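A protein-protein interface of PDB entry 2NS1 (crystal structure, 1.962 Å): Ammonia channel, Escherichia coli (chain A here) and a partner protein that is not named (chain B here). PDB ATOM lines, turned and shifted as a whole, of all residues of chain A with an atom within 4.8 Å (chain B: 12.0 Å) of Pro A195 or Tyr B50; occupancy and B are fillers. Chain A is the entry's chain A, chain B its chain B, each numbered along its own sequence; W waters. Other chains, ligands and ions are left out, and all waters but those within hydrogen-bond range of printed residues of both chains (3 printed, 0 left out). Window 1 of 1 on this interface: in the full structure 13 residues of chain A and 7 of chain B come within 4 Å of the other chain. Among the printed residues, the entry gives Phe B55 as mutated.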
ATOM      1  N   GLY A  34      12.210  -8.072 -16.798  1.00  0.00           N
ATOM      2  CA  GLY A  34      12.679  -9.064 -17.789  1.00  0.00           C
ATOM      3  C   GLY A  34      13.795  -9.974 -17.301  1.00  0.00           C
ATOM      4  O   GLY A  34      13.970 -11.062 -17.820  1.00  0.00           O
ATOM      5  N   LEU A  35      14.580  -9.486 -16.340  1.00  0.00           N
ATOM      6  CA  LEU A  35      15.732 -10.206 -15.802  1.00  0.00           C
ATOM      7  C   LEU A  35      15.341 -11.337 -14.876  1.00  0.00           C
ATOM      8  O   LEU A  35      16.126 -12.263 -14.678  1.00  0.00           O
ATOM      9  CB  LEU A  35      16.640  -9.248 -15.019  1.00  0.00           C
ATOM     10  CG  LEU A  35      17.491  -8.315 -15.860  1.00  0.00           C
ATOM     11  CD1 LEU A  35      18.237  -7.323 -14.963  1.00  0.00           C
ATOM     12  CD2 LEU A  35      18.436  -9.120 -16.752  1.00  0.00           C
ATOM     13  N   ILE A  36      14.157 -11.251 -14.279  1.00  0.00           N
ATOM     14  CA  ILE A  36      13.705 -12.273 -13.320  1.00  0.00           C
ATOM     15  C   ILE A  36      12.734 -13.242 -13.973  1.00  0.00           C
ATOM     16  O   ILE A  36      12.473 -13.162 -15.177  1.00  0.00           O
ATOM     17  CB  ILE A  36      13.150 -11.628 -12.012  1.00  0.00           C
ATOM     18  CG1 ILE A  36      11.823 -10.869 -12.233  1.00  0.00           C
ATOM     19  CG2 ILE A  36      14.211 -10.706 -11.396  1.00  0.00           C
ATOM     20  CD1 ILE A  36      11.314 -10.191 -10.969  1.00  0.00           C
ATOM     21  N   PHE A 193      18.242 -19.701 -12.961  1.00  0.00           N
ATOM     22  CA  PHE A 193      17.488 -18.467 -13.054  1.00  0.00           C
ATOM     23  C   PHE A 193      17.909 -17.724 -14.315  1.00  0.00           C
ATOM     24  O   PHE A 193      18.829 -16.938 -14.309  1.00  0.00           O
ATOM     25  CB  PHE A 193      17.692 -17.602 -11.815  1.00  0.00           C
ATOM     26  CG  PHE A 193      17.457 -18.324 -10.524  1.00  0.00           C
ATOM     27  CD1 PHE A 193      16.353 -19.149 -10.357  1.00  0.00           C
ATOM     28  CD2 PHE A 193      18.341 -18.179  -9.471  1.00  0.00           C
ATOM     29  CE1 PHE A 193      16.144 -19.820  -9.155  1.00  0.00           C
ATOM     30  CE2 PHE A 193      18.130 -18.840  -8.270  1.00  0.00           C
ATOM     31  CZ  PHE A 193      17.026 -19.662  -8.117  1.00  0.00           C
ATOM     32  N   LYS A 194      17.234 -18.009 -15.416  1.00  0.00           N
ATOM     33  CA  LYS A 194      17.460 -17.284 -16.646  1.00  0.00           C
ATOM     34  C   LYS A 194      16.525 -16.077 -16.690  1.00  0.00           C
ATOM     35  O   LYS A 194      15.438 -16.095 -16.106  1.00  0.00           O
ATOM     36  CB  LYS A 194      17.168 -18.200 -17.841  1.00  0.00           C
ATOM     37  CG  LYS A 194      18.144 -19.306 -18.047  1.00  0.00           C
ATOM     38  CD  LYS A 194      17.727 -20.147 -19.238  1.00  0.00           C
ATOM     39  CE  LYS A 194      18.668 -21.324 -19.446  1.00  0.00           C
ATOM     40  NZ  LYS A 194      18.340 -22.053 -20.670  1.00  0.00           N
ATOM     41  N   PRO A 195      16.917 -15.017 -17.417  1.00  0.00           N
ATOM     42  CA  PRO A 195      15.943 -13.929 -17.578  1.00  0.00           C
ATOM     43  C   PRO A 195      14.722 -14.414 -18.348  1.00  0.00           C
ATOM     44  O   PRO A 195      14.865 -15.104 -19.383  1.00  0.00           O
ATOM     45  CB  PRO A 195      16.711 -12.869 -18.360  1.00  0.00           C
ATOM     46  CG  PRO A 195      17.913 -13.535 -18.890  1.00  0.00           C
ATOM     47  CD  PRO A 195      18.183 -14.763 -18.112  1.00  0.00           C
ATOM     48  N   HIS A 196      13.522 -14.100 -17.869  1.00  0.00           N
ATOM     49  CA  HIS A 196      12.342 -14.640 -18.555  1.00  0.00           C
ATOM     50  C   HIS A 196      12.049 -13.964 -19.888  1.00  0.00           C
ATOM     51  O   HIS A 196      11.468 -14.583 -20.772  1.00  0.00           O
ATOM     52  CB  HIS A 196      11.099 -14.691 -17.648  1.00  0.00           C
ATOM     53  CG  HIS A 196      10.211 -13.480 -17.734  1.00  0.00           C
ATOM     54  ND1 HIS A 196      10.488 -12.303 -17.062  1.00  0.00           N
ATOM     55  CD2 HIS A 196       9.037 -13.282 -18.371  1.00  0.00           C
ATOM     56  CE1 HIS A 196       9.510 -11.434 -17.279  1.00  0.00           C
ATOM     57  NE2 HIS A 196       8.630 -11.992 -18.093  1.00  0.00           N
ATOM     58  N   ASN A 197      12.460 -12.711 -20.055  1.00  0.00           N
ATOM     59  CA  ASN A 197      12.105 -11.970 -21.268  1.00  0.00           C
ATOM     60  C   ASN A 197      13.183 -10.953 -21.605  1.00  0.00           C
ATOM     61  O   ASN A 197      13.169  -9.842 -21.080  1.00  0.00           O
ATOM     62  CB  ASN A 197      10.749 -11.292 -21.075  1.00  0.00           C
ATOM     63  CG  ASN A 197      10.194 -10.706 -22.352  1.00  0.00           C
ATOM     64  OD1 ASN A 197      10.938 -10.271 -23.217  1.00  0.00           O
ATOM     65  ND2 ASN A 197       8.874 -10.696 -22.472  1.00  0.00           N
ATOM     66  N   LEU A 198      14.107 -11.316 -22.478  1.00  0.00           N
ATOM     67  CA  LEU A 198      15.226 -10.429 -22.792  1.00  0.00           C
ATOM     68  C   LEU A 198      14.780  -9.215 -23.644  1.00  0.00           C
ATOM     69  O   LEU A 198      15.328  -8.134 -23.462  1.00  0.00           O
ATOM     70  CB  LEU A 198      16.421 -11.169 -23.409  1.00  0.00           C
ATOM     71  CG  LEU A 198      17.352 -11.860 -22.389  1.00  0.00           C
ATOM     72  CD1 LEU A 198      18.392 -12.742 -23.072  1.00  0.00           C
ATOM     73  CD2 LEU A 198      18.039 -10.812 -21.440  1.00  0.00           C
ATOM     74  N   ARG A 253      34.719 -14.567 -23.013  1.00  0.00           N
ATOM     75  CA  ARG A 253      33.690 -15.616 -22.913  1.00  0.00           C
ATOM     76  C   ARG A 253      33.307 -16.217 -24.264  1.00  0.00           C
ATOM     77  O   ARG A 253      32.705 -17.278 -24.327  1.00  0.00           O
ATOM     78  CB  ARG A 253      32.464 -15.064 -22.201  1.00  0.00           C
ATOM     79  CG  ARG A 253      32.758 -14.601 -20.782  1.00  0.00           C
ATOM     80  CD  ARG A 253      31.818 -13.497 -20.311  1.00  0.00           C
ATOM     81  NE  ARG A 253      30.405 -13.871 -20.422  1.00  0.00           N
ATOM     82  CZ  ARG A 253      29.392 -13.238 -19.820  1.00  0.00           C
ATOM     83  NH1 ARG A 253      29.595 -12.182 -19.034  1.00  0.00           N
ATOM     84  NH2 ARG A 253      28.155 -13.677 -20.004  1.00  0.00           N
ATOM     85  N   LEU A 259      22.226  -9.176 -23.541  1.00  0.00           N
ATOM     86  CA  LEU A 259      22.251  -8.704 -22.172  1.00  0.00           C
ATOM     87  C   LEU A 259      23.565  -7.966 -21.817  1.00  0.00           C
ATOM     88  O   LEU A 259      23.577  -6.997 -21.022  1.00  0.00           O
ATOM     89  CB  LEU A 259      21.977  -9.871 -21.226  1.00  0.00           C
ATOM     90  CG  LEU A 259      21.890  -9.528 -19.748  1.00  0.00           C
ATOM     91  CD1 LEU A 259      20.889  -8.419 -19.485  1.00  0.00           C
ATOM     92  CD2 LEU A 259      21.511 -10.797 -18.980  1.00  0.00           C
ATOM     93  N   GLY B  45      21.693 -28.823 -26.364  1.00  0.00           N
ATOM     94  CA  GLY B  45      21.687 -27.379 -26.583  1.00  0.00           C
ATOM     95  C   GLY B  45      23.049 -26.730 -26.370  1.00  0.00           C
ATOM     96  O   GLY B  45      23.865 -27.205 -25.566  1.00  0.00           O
ATOM     97  N   HIS B  46      23.304 -25.641 -27.095  1.00  0.00           N
ATOM     98  CA  HIS B  46      24.521 -24.853 -26.886  1.00  0.00           C
ATOM     99  C   HIS B  46      24.486 -24.330 -25.454  1.00  0.00           C
ATOM    100  O   HIS B  46      23.412 -24.245 -24.860  1.00  0.00           O
ATOM    101  CB  HIS B  46      24.572 -23.652 -27.845  1.00  0.00           C
ATOM    102  CG  HIS B  46      24.782 -24.011 -29.284  1.00  0.00           C
ATOM    103  ND1 HIS B  46      23.869 -24.740 -30.014  1.00  0.00           N
ATOM    104  CD2 HIS B  46      25.777 -23.688 -30.144  1.00  0.00           C
ATOM    105  CE1 HIS B  46      24.306 -24.878 -31.254  1.00  0.00           C
ATOM    106  NE2 HIS B  46      25.462 -24.249 -31.362  1.00  0.00           N
ATOM    107  N   ALA B  47      25.644 -23.959 -24.906  1.00  0.00           N
ATOM    108  CA  ALA B  47      25.697 -23.254 -23.630  1.00  0.00           C
ATOM    109  C   ALA B  47      25.061 -21.868 -23.812  1.00  0.00           C
ATOM    110  O   ALA B  47      25.079 -21.299 -24.908  1.00  0.00           O
ATOM    111  CB  ALA B  47      27.126 -23.095 -23.146  1.00  0.00           C
ATOM    112  N   GLU B  48      24.499 -21.348 -22.734  1.00  0.00           N
ATOM    113  CA  GLU B  48      23.947 -19.994 -22.719  1.00  0.00           C
ATOM    114  C   GLU B  48      24.585 -19.263 -21.554  1.00  0.00           C
ATOM    115  O   GLU B  48      24.877 -19.859 -20.520  1.00  0.00           O
ATOM    116  CB  GLU B  48      22.441 -20.042 -22.538  1.00  0.00           C
ATOM    117  CG  GLU B  48      21.695 -20.670 -23.694  1.00  0.00           C
ATOM    118  CD  GLU B  48      20.204 -20.862 -23.428  1.00  0.00           C
ATOM    119  OE1 GLU B  48      19.661 -20.290 -22.445  1.00  0.00           O
ATOM    120  OE2 GLU B  48      19.573 -21.608 -24.217  1.00  0.00           O
ATOM    121  N   LEU B  49      24.801 -17.972 -21.723  1.00  0.00           N
ATOM    122  CA  LEU B  49      25.397 -17.155 -20.689  1.00  0.00           C
ATOM    123  C   LEU B  49      24.599 -15.901 -20.505  1.00  0.00           C
ATOM    124  O   LEU B  49      24.251 -15.258 -21.487  1.00  0.00           O
ATOM    125  CB  LEU B  49      26.803 -16.754 -21.091  1.00  0.00           C
ATOM    126  CG  LEU B  49      27.878 -17.813 -21.174  1.00  0.00           C
ATOM    127  CD1 LEU B  49      29.200 -17.106 -21.436  1.00  0.00           C
ATOM    128  CD2 LEU B  49      27.939 -18.589 -19.886  1.00  0.00           C
ATOM    129  N   TYR B  50      24.313 -15.568 -19.250  1.00  0.00           N
ATOM    130  CA  TYR B  50      23.564 -14.372 -18.906  1.00  0.00           C
ATOM    131  C   TYR B  50      24.322 -13.672 -17.793  1.00  0.00           C
ATOM    132  O   TYR B  50      24.329 -14.139 -16.638  1.00  0.00           O
ATOM    133  CB  TYR B  50      22.162 -14.764 -18.449  1.00  0.00           C
ATOM    134  CG  TYR B  50      21.397 -15.541 -19.488  1.00  0.00           C
ATOM    135  CD1 TYR B  50      20.711 -14.890 -20.514  1.00  0.00           C
ATOM    136  CD2 TYR B  50      21.366 -16.931 -19.461  1.00  0.00           C
ATOM    137  CE1 TYR B  50      19.998 -15.604 -21.454  1.00  0.00           C
ATOM    138  CE2 TYR B  50      20.667 -17.651 -20.413  1.00  0.00           C
ATOM    139  CZ  TYR B  50      19.986 -16.977 -21.408  1.00  0.00           C
ATOM    140  OH  TYR B  50      19.320 -17.686 -22.376  1.00  0.00           O
ATOM    141  N   ARG B  51      25.030 -12.602 -18.144  1.00  0.00           N
ATOM    142  CA  ARG B  51      25.948 -11.953 -17.194  1.00  0.00           C
ATOM    143  C   ARG B  51      26.846 -13.030 -16.543  1.00  0.00           C
ATOM    144  O   ARG B  51      27.494 -13.801 -17.266  1.00  0.00           O
ATOM    145  CB  ARG B  51      25.147 -11.117 -16.201  1.00  0.00           C
ATOM    146  CG  ARG B  51      24.539  -9.845 -16.849  1.00  0.00           C
ATOM    147  CD  ARG B  51      23.515  -9.197 -15.935  1.00  0.00           C
ATOM    148  NE  ARG B  51      23.341  -7.786 -16.251  1.00  0.00           N
ATOM    149  CZ  ARG B  51      22.618  -6.947 -15.525  1.00  0.00           C
ATOM    150  NH1 ARG B  51      21.993  -7.365 -14.445  1.00  0.00           N
ATOM    151  NH2 ARG B  51      22.507  -5.668 -15.887  1.00  0.00           N
ATOM    152  N   GLY B  52      26.877 -13.126 -15.221  1.00  0.00           N
ATOM    153  CA  GLY B  52      27.721 -14.123 -14.561  1.00  0.00           C
ATOM    154  C   GLY B  52      27.231 -15.558 -14.617  1.00  0.00           C
ATOM    155  O   GLY B  52      27.976 -16.468 -14.259  1.00  0.00           O
ATOM    156  N   ALA B  53      25.990 -15.770 -15.050  1.00  0.00           N
ATOM    157  CA  ALA B  53      25.355 -17.103 -14.998  1.00  0.00           C
ATOM    158  C   ALA B  53      25.608 -17.886 -16.268  1.00  0.00           C
ATOM    159  O   ALA B  53      25.365 -17.399 -17.368  1.00  0.00           O
ATOM    160  CB  ALA B  53      23.844 -16.987 -14.744  1.00  0.00           C
ATOM    161  N   GLU B  54      26.088 -19.120 -16.107  1.00  0.00           N
ATOM    162  CA  GLU B  54      26.432 -19.996 -17.218  1.00  0.00           C
ATOM    163  C   GLU B  54      25.498 -21.192 -17.164  1.00  0.00           C
ATOM    164  O   GLU B  54      25.243 -21.721 -16.076  1.00  0.00           O
ATOM    165  CB  GLU B  54      27.886 -20.427 -17.068  1.00  0.00           C
ATOM    166  CG  GLU B  54      28.401 -21.402 -18.098  1.00  0.00           C
ATOM    167  CD  GLU B  54      29.920 -21.572 -17.999  1.00  0.00           C
ATOM    168  OE1 GLU B  54      30.413 -21.881 -16.887  1.00  0.00           O
ATOM    169  OE2 GLU B  54      30.612 -21.384 -19.029  1.00  0.00           O
ATOM    170  N   PHE B  55      24.952 -21.583 -18.316  1.00  0.00           N
ATOM    171  CA  PHE B  55      24.036 -22.734 -18.400  1.00  0.00           C
ATOM    172  C   PHE B  55      24.527 -23.640 -19.502  1.00  0.00           C
ATOM    173  O   PHE B  55      24.445 -23.301 -20.681  1.00  0.00           O
ATOM    174  CB  PHE B  55      22.598 -22.299 -18.673  1.00  0.00           C
ATOM    175  CG  PHE B  55      22.047 -21.407 -17.623  1.00  0.00           C
ATOM    176  CD1 PHE B  55      21.389 -21.933 -16.532  1.00  0.00           C
ATOM    177  CD2 PHE B  55      22.243 -20.042 -17.680  1.00  0.00           C
ATOM    178  CE1 PHE B  55      20.932 -21.109 -15.536  1.00  0.00           C
ATOM    179  CE2 PHE B  55      21.777 -19.220 -16.680  1.00  0.00           C
ATOM    180  CZ  PHE B  55      21.115 -19.754 -15.615  1.00  0.00           C
ATOM    181  N   SER B  56      25.058 -24.791 -19.114  1.00  0.00           N
ATOM    182  CA  SER B  56      25.723 -25.677 -20.058  1.00  0.00           C
ATOM    183  C   SER B  56      24.789 -26.792 -20.490  1.00  0.00           C
ATOM    184  O   SER B  56      25.069 -27.492 -21.459  1.00  0.00           O
ATOM    185  CB  SER B  56      26.994 -26.255 -19.430  1.00  0.00           C
ATOM    186  OG  SER B  56      26.684 -26.939 -18.233  1.00  0.00           O
ATOM    187  N   VAL B  57      23.686 -26.961 -19.761  1.00  0.00           N
ATOM    188  CA  VAL B  57      22.680 -27.970 -20.084  1.00  0.00           C
ATOM    189  C   VAL B  57      21.439 -27.228 -20.535  1.00  0.00           C
ATOM    190  O   VAL B  57      20.855 -26.493 -19.739  1.00  0.00           O
ATOM    191  CB  VAL B  57      22.320 -28.867 -18.853  1.00  0.00           C
ATOM    192  CG1 VAL B  57      21.279 -29.920 -19.229  1.00  0.00           C
ATOM    193  CG2 VAL B  57      23.570 -29.531 -18.268  1.00  0.00           C
ATOM    194  N   ASN B  58      21.056 -27.395 -21.806  1.00  0.00           N
ATOM    195  CA  ASN B  58      19.846 -26.774 -22.333  1.00  0.00           C
ATOM    196  C   ASN B  58      19.051 -27.733 -23.224  1.00  0.00           C
ATOM    197  O   ASN B  58      19.630 -28.548 -23.950  1.00  0.00           O
ATOM    198  CB  ASN B  58      20.197 -25.474 -23.079  1.00  0.00           C
ATOM    199  CG  ASN B  58      20.829 -24.436 -22.160  1.00  0.00           C
ATOM    200  OD1 ASN B  58      20.274 -24.094 -21.112  1.00  0.00           O
ATOM    201  ND2 ASN B  58      21.998 -23.965 -22.525  1.00  0.00           N
ATOM    202  N   PHE B  59      17.720 -27.640 -23.144  1.00  0.00           N
ATOM    203  CA  PHE B  59      16.821 -28.436 -24.000  1.00  0.00           C
ATOM    204  C   PHE B  59      16.909 -27.968 -25.451  1.00  0.00           C
ATOM    205  O   PHE B  59      17.385 -26.866 -25.712  1.00  0.00           O
ATOM    206  CB  PHE B  59      15.371 -28.263 -23.537  1.00  0.00           C
ATOM    207  CG  PHE B  59      14.797 -26.870 -23.824  1.00  0.00           C
ATOM    208  CD1 PHE B  59      14.648 -25.936 -22.800  1.00  0.00           C
ATOM    209  CD2 PHE B  59      14.414 -26.493 -25.117  1.00  0.00           C
ATOM    210  CE1 PHE B  59      14.126 -24.651 -23.056  1.00  0.00           C
ATOM    211  CE2 PHE B  59      13.896 -25.209 -25.381  1.00  0.00           C
ATOM    212  CZ  PHE B  59      13.754 -24.291 -24.345  1.00  0.00           C
ATOM    213  N   PRO B  61      14.087 -27.246 -28.708  1.00  0.00           N
ATOM    214  CA  PRO B  61      12.684 -27.263 -29.096  1.00  0.00           C
ATOM    215  C   PRO B  61      12.436 -28.399 -30.082  1.00  0.00           C
ATOM    216  O   PRO B  61      13.261 -28.658 -30.949  1.00  0.00           O
ATOM    217  CB  PRO B  61      12.492 -25.917 -29.791  1.00  0.00           C
ATOM    218  CG  PRO B  61      13.861 -25.551 -30.281  1.00  0.00           C
ATOM    219  CD  PRO B  61      14.768 -26.032 -29.188  1.00  0.00           C
HETATM  220  O   HOH W   1      25.537 -11.486 -20.526  1.00  0.00           O
HETATM  221  O   HOH W   2      17.249 -22.684 -23.911  1.00  0.00           O
HETATM  222  O   HOH W   3      30.102 -15.206 -17.626  1.00  0.00           O
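The backbone carbonyl oxygen of Arg B51 lies within hydrogen-bond range of the guanidinium group of Arg A253 (2.8 Å).
The side-chain amino group of Lys A194 lies within hydrogen-bond range of the side-chain amide oxygen of Asn B58 (2.8 Å).
NZ of Lys A194 lies within salt-bridge range of OE1 of Glu B48 (2.8 Å).
O of Glu B48 lies within hydrogen-bond range of N of Phe B55 (2.8 Å).
O of His B46 is in hydrogen-bond range of ND2 of Asn B58, at 2.7 Å.
The backbone carbonyl oxygen of Phe B55 lies within hydrogen-bond range of the side-chain amide nitrogen of Asn B58, 3.1 Å away.
The backbone NH (N) of Gly B45 is in hydrogen-bond range of the backbone carbonyl oxygen (O) of Asn B58.
OH of Tyr B50 sits at hydrogen-bond distance from OE1 of Glu B48 (2.6 Å).
Among the printed residues, pairs that only touch across the chains: Pro A195 with Tyr B50 (3.5 Å), Arg A253 with Leu B49 (3.5 Å), Leu A198 with Tyr B50 (3.7 Å), Leu A35 with Arg B51 (3.8 Å), Leu A259 with Arg B51 (3.8 Å), Lys A194 with Tyr B50 (3.8 Å), Lys A194 with Phe B55 (3.8 Å) and Phe A193 with Phe B55 (3.9 Å).
Gly A34 touches none of the printed residues of chain B.
Ile A36 touches none of the printed residues of chain B.
Printed residues of chain B within 4 Å of Phe A193: Phe B55 (3.9 Å).
Pro A195 touches one residue of chain B.
No residue of chain B comes within 4 Å of His A196.
Of the printed residues of chain B, Leu A198 touches Tyr B50.
Of the printed residues of chain A, Leu B49 touches Arg A253.
Of chain A, only Lys A194 (3.8 Å), Pro A195 (3.5 Å) and Leu A198 (3.7 Å) come within 4 Å of Tyr B50.
Of the printed residues of chain A, Arg B51 touches Leu A35 (3.8 Å), Arg A253 (2.8 Å) and Leu A259 (3.8 Å).
Of the printed residues of chain A, Phe B55 touches Phe A193 and Lys A194.
Printed residues of chain A within 4 Å of Asn B58: Lys A194 (2.8 Å).
The nearest residue of chain A that does not touch Tyr B50 is Leu A259 (4.1 Å).
Of the 16 printed residues of chain B, 6 touch a printed residue of chain A.
Hydrophobic or aromatic side chains of chain B that line the printed part of chain A: Leu B49, Tyr B50 and Phe B55.
Of the 11 printed residues of chain A, 7 touch a printed residue of chain B.
Among the printed residues, Asp or Glu carboxylates within 4 Å of a Lys or Arg side-chain nitrogen of the other chain: Lys A194 with Glu B48.
Water W2 bridges OE2 of Glu B48 and NZ of Lys A194.
Water W1 bridges the backbone NH (N) of Arg B51 (2.7 Å) and the guanidinium group (NH2) of Arg A253 (3.5 Å).
Water W3 bridges the backbone carbonyl oxygen of Arg B51 (3.0 Å) and the guanidinium group of Arg A253 (3.1 Å).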
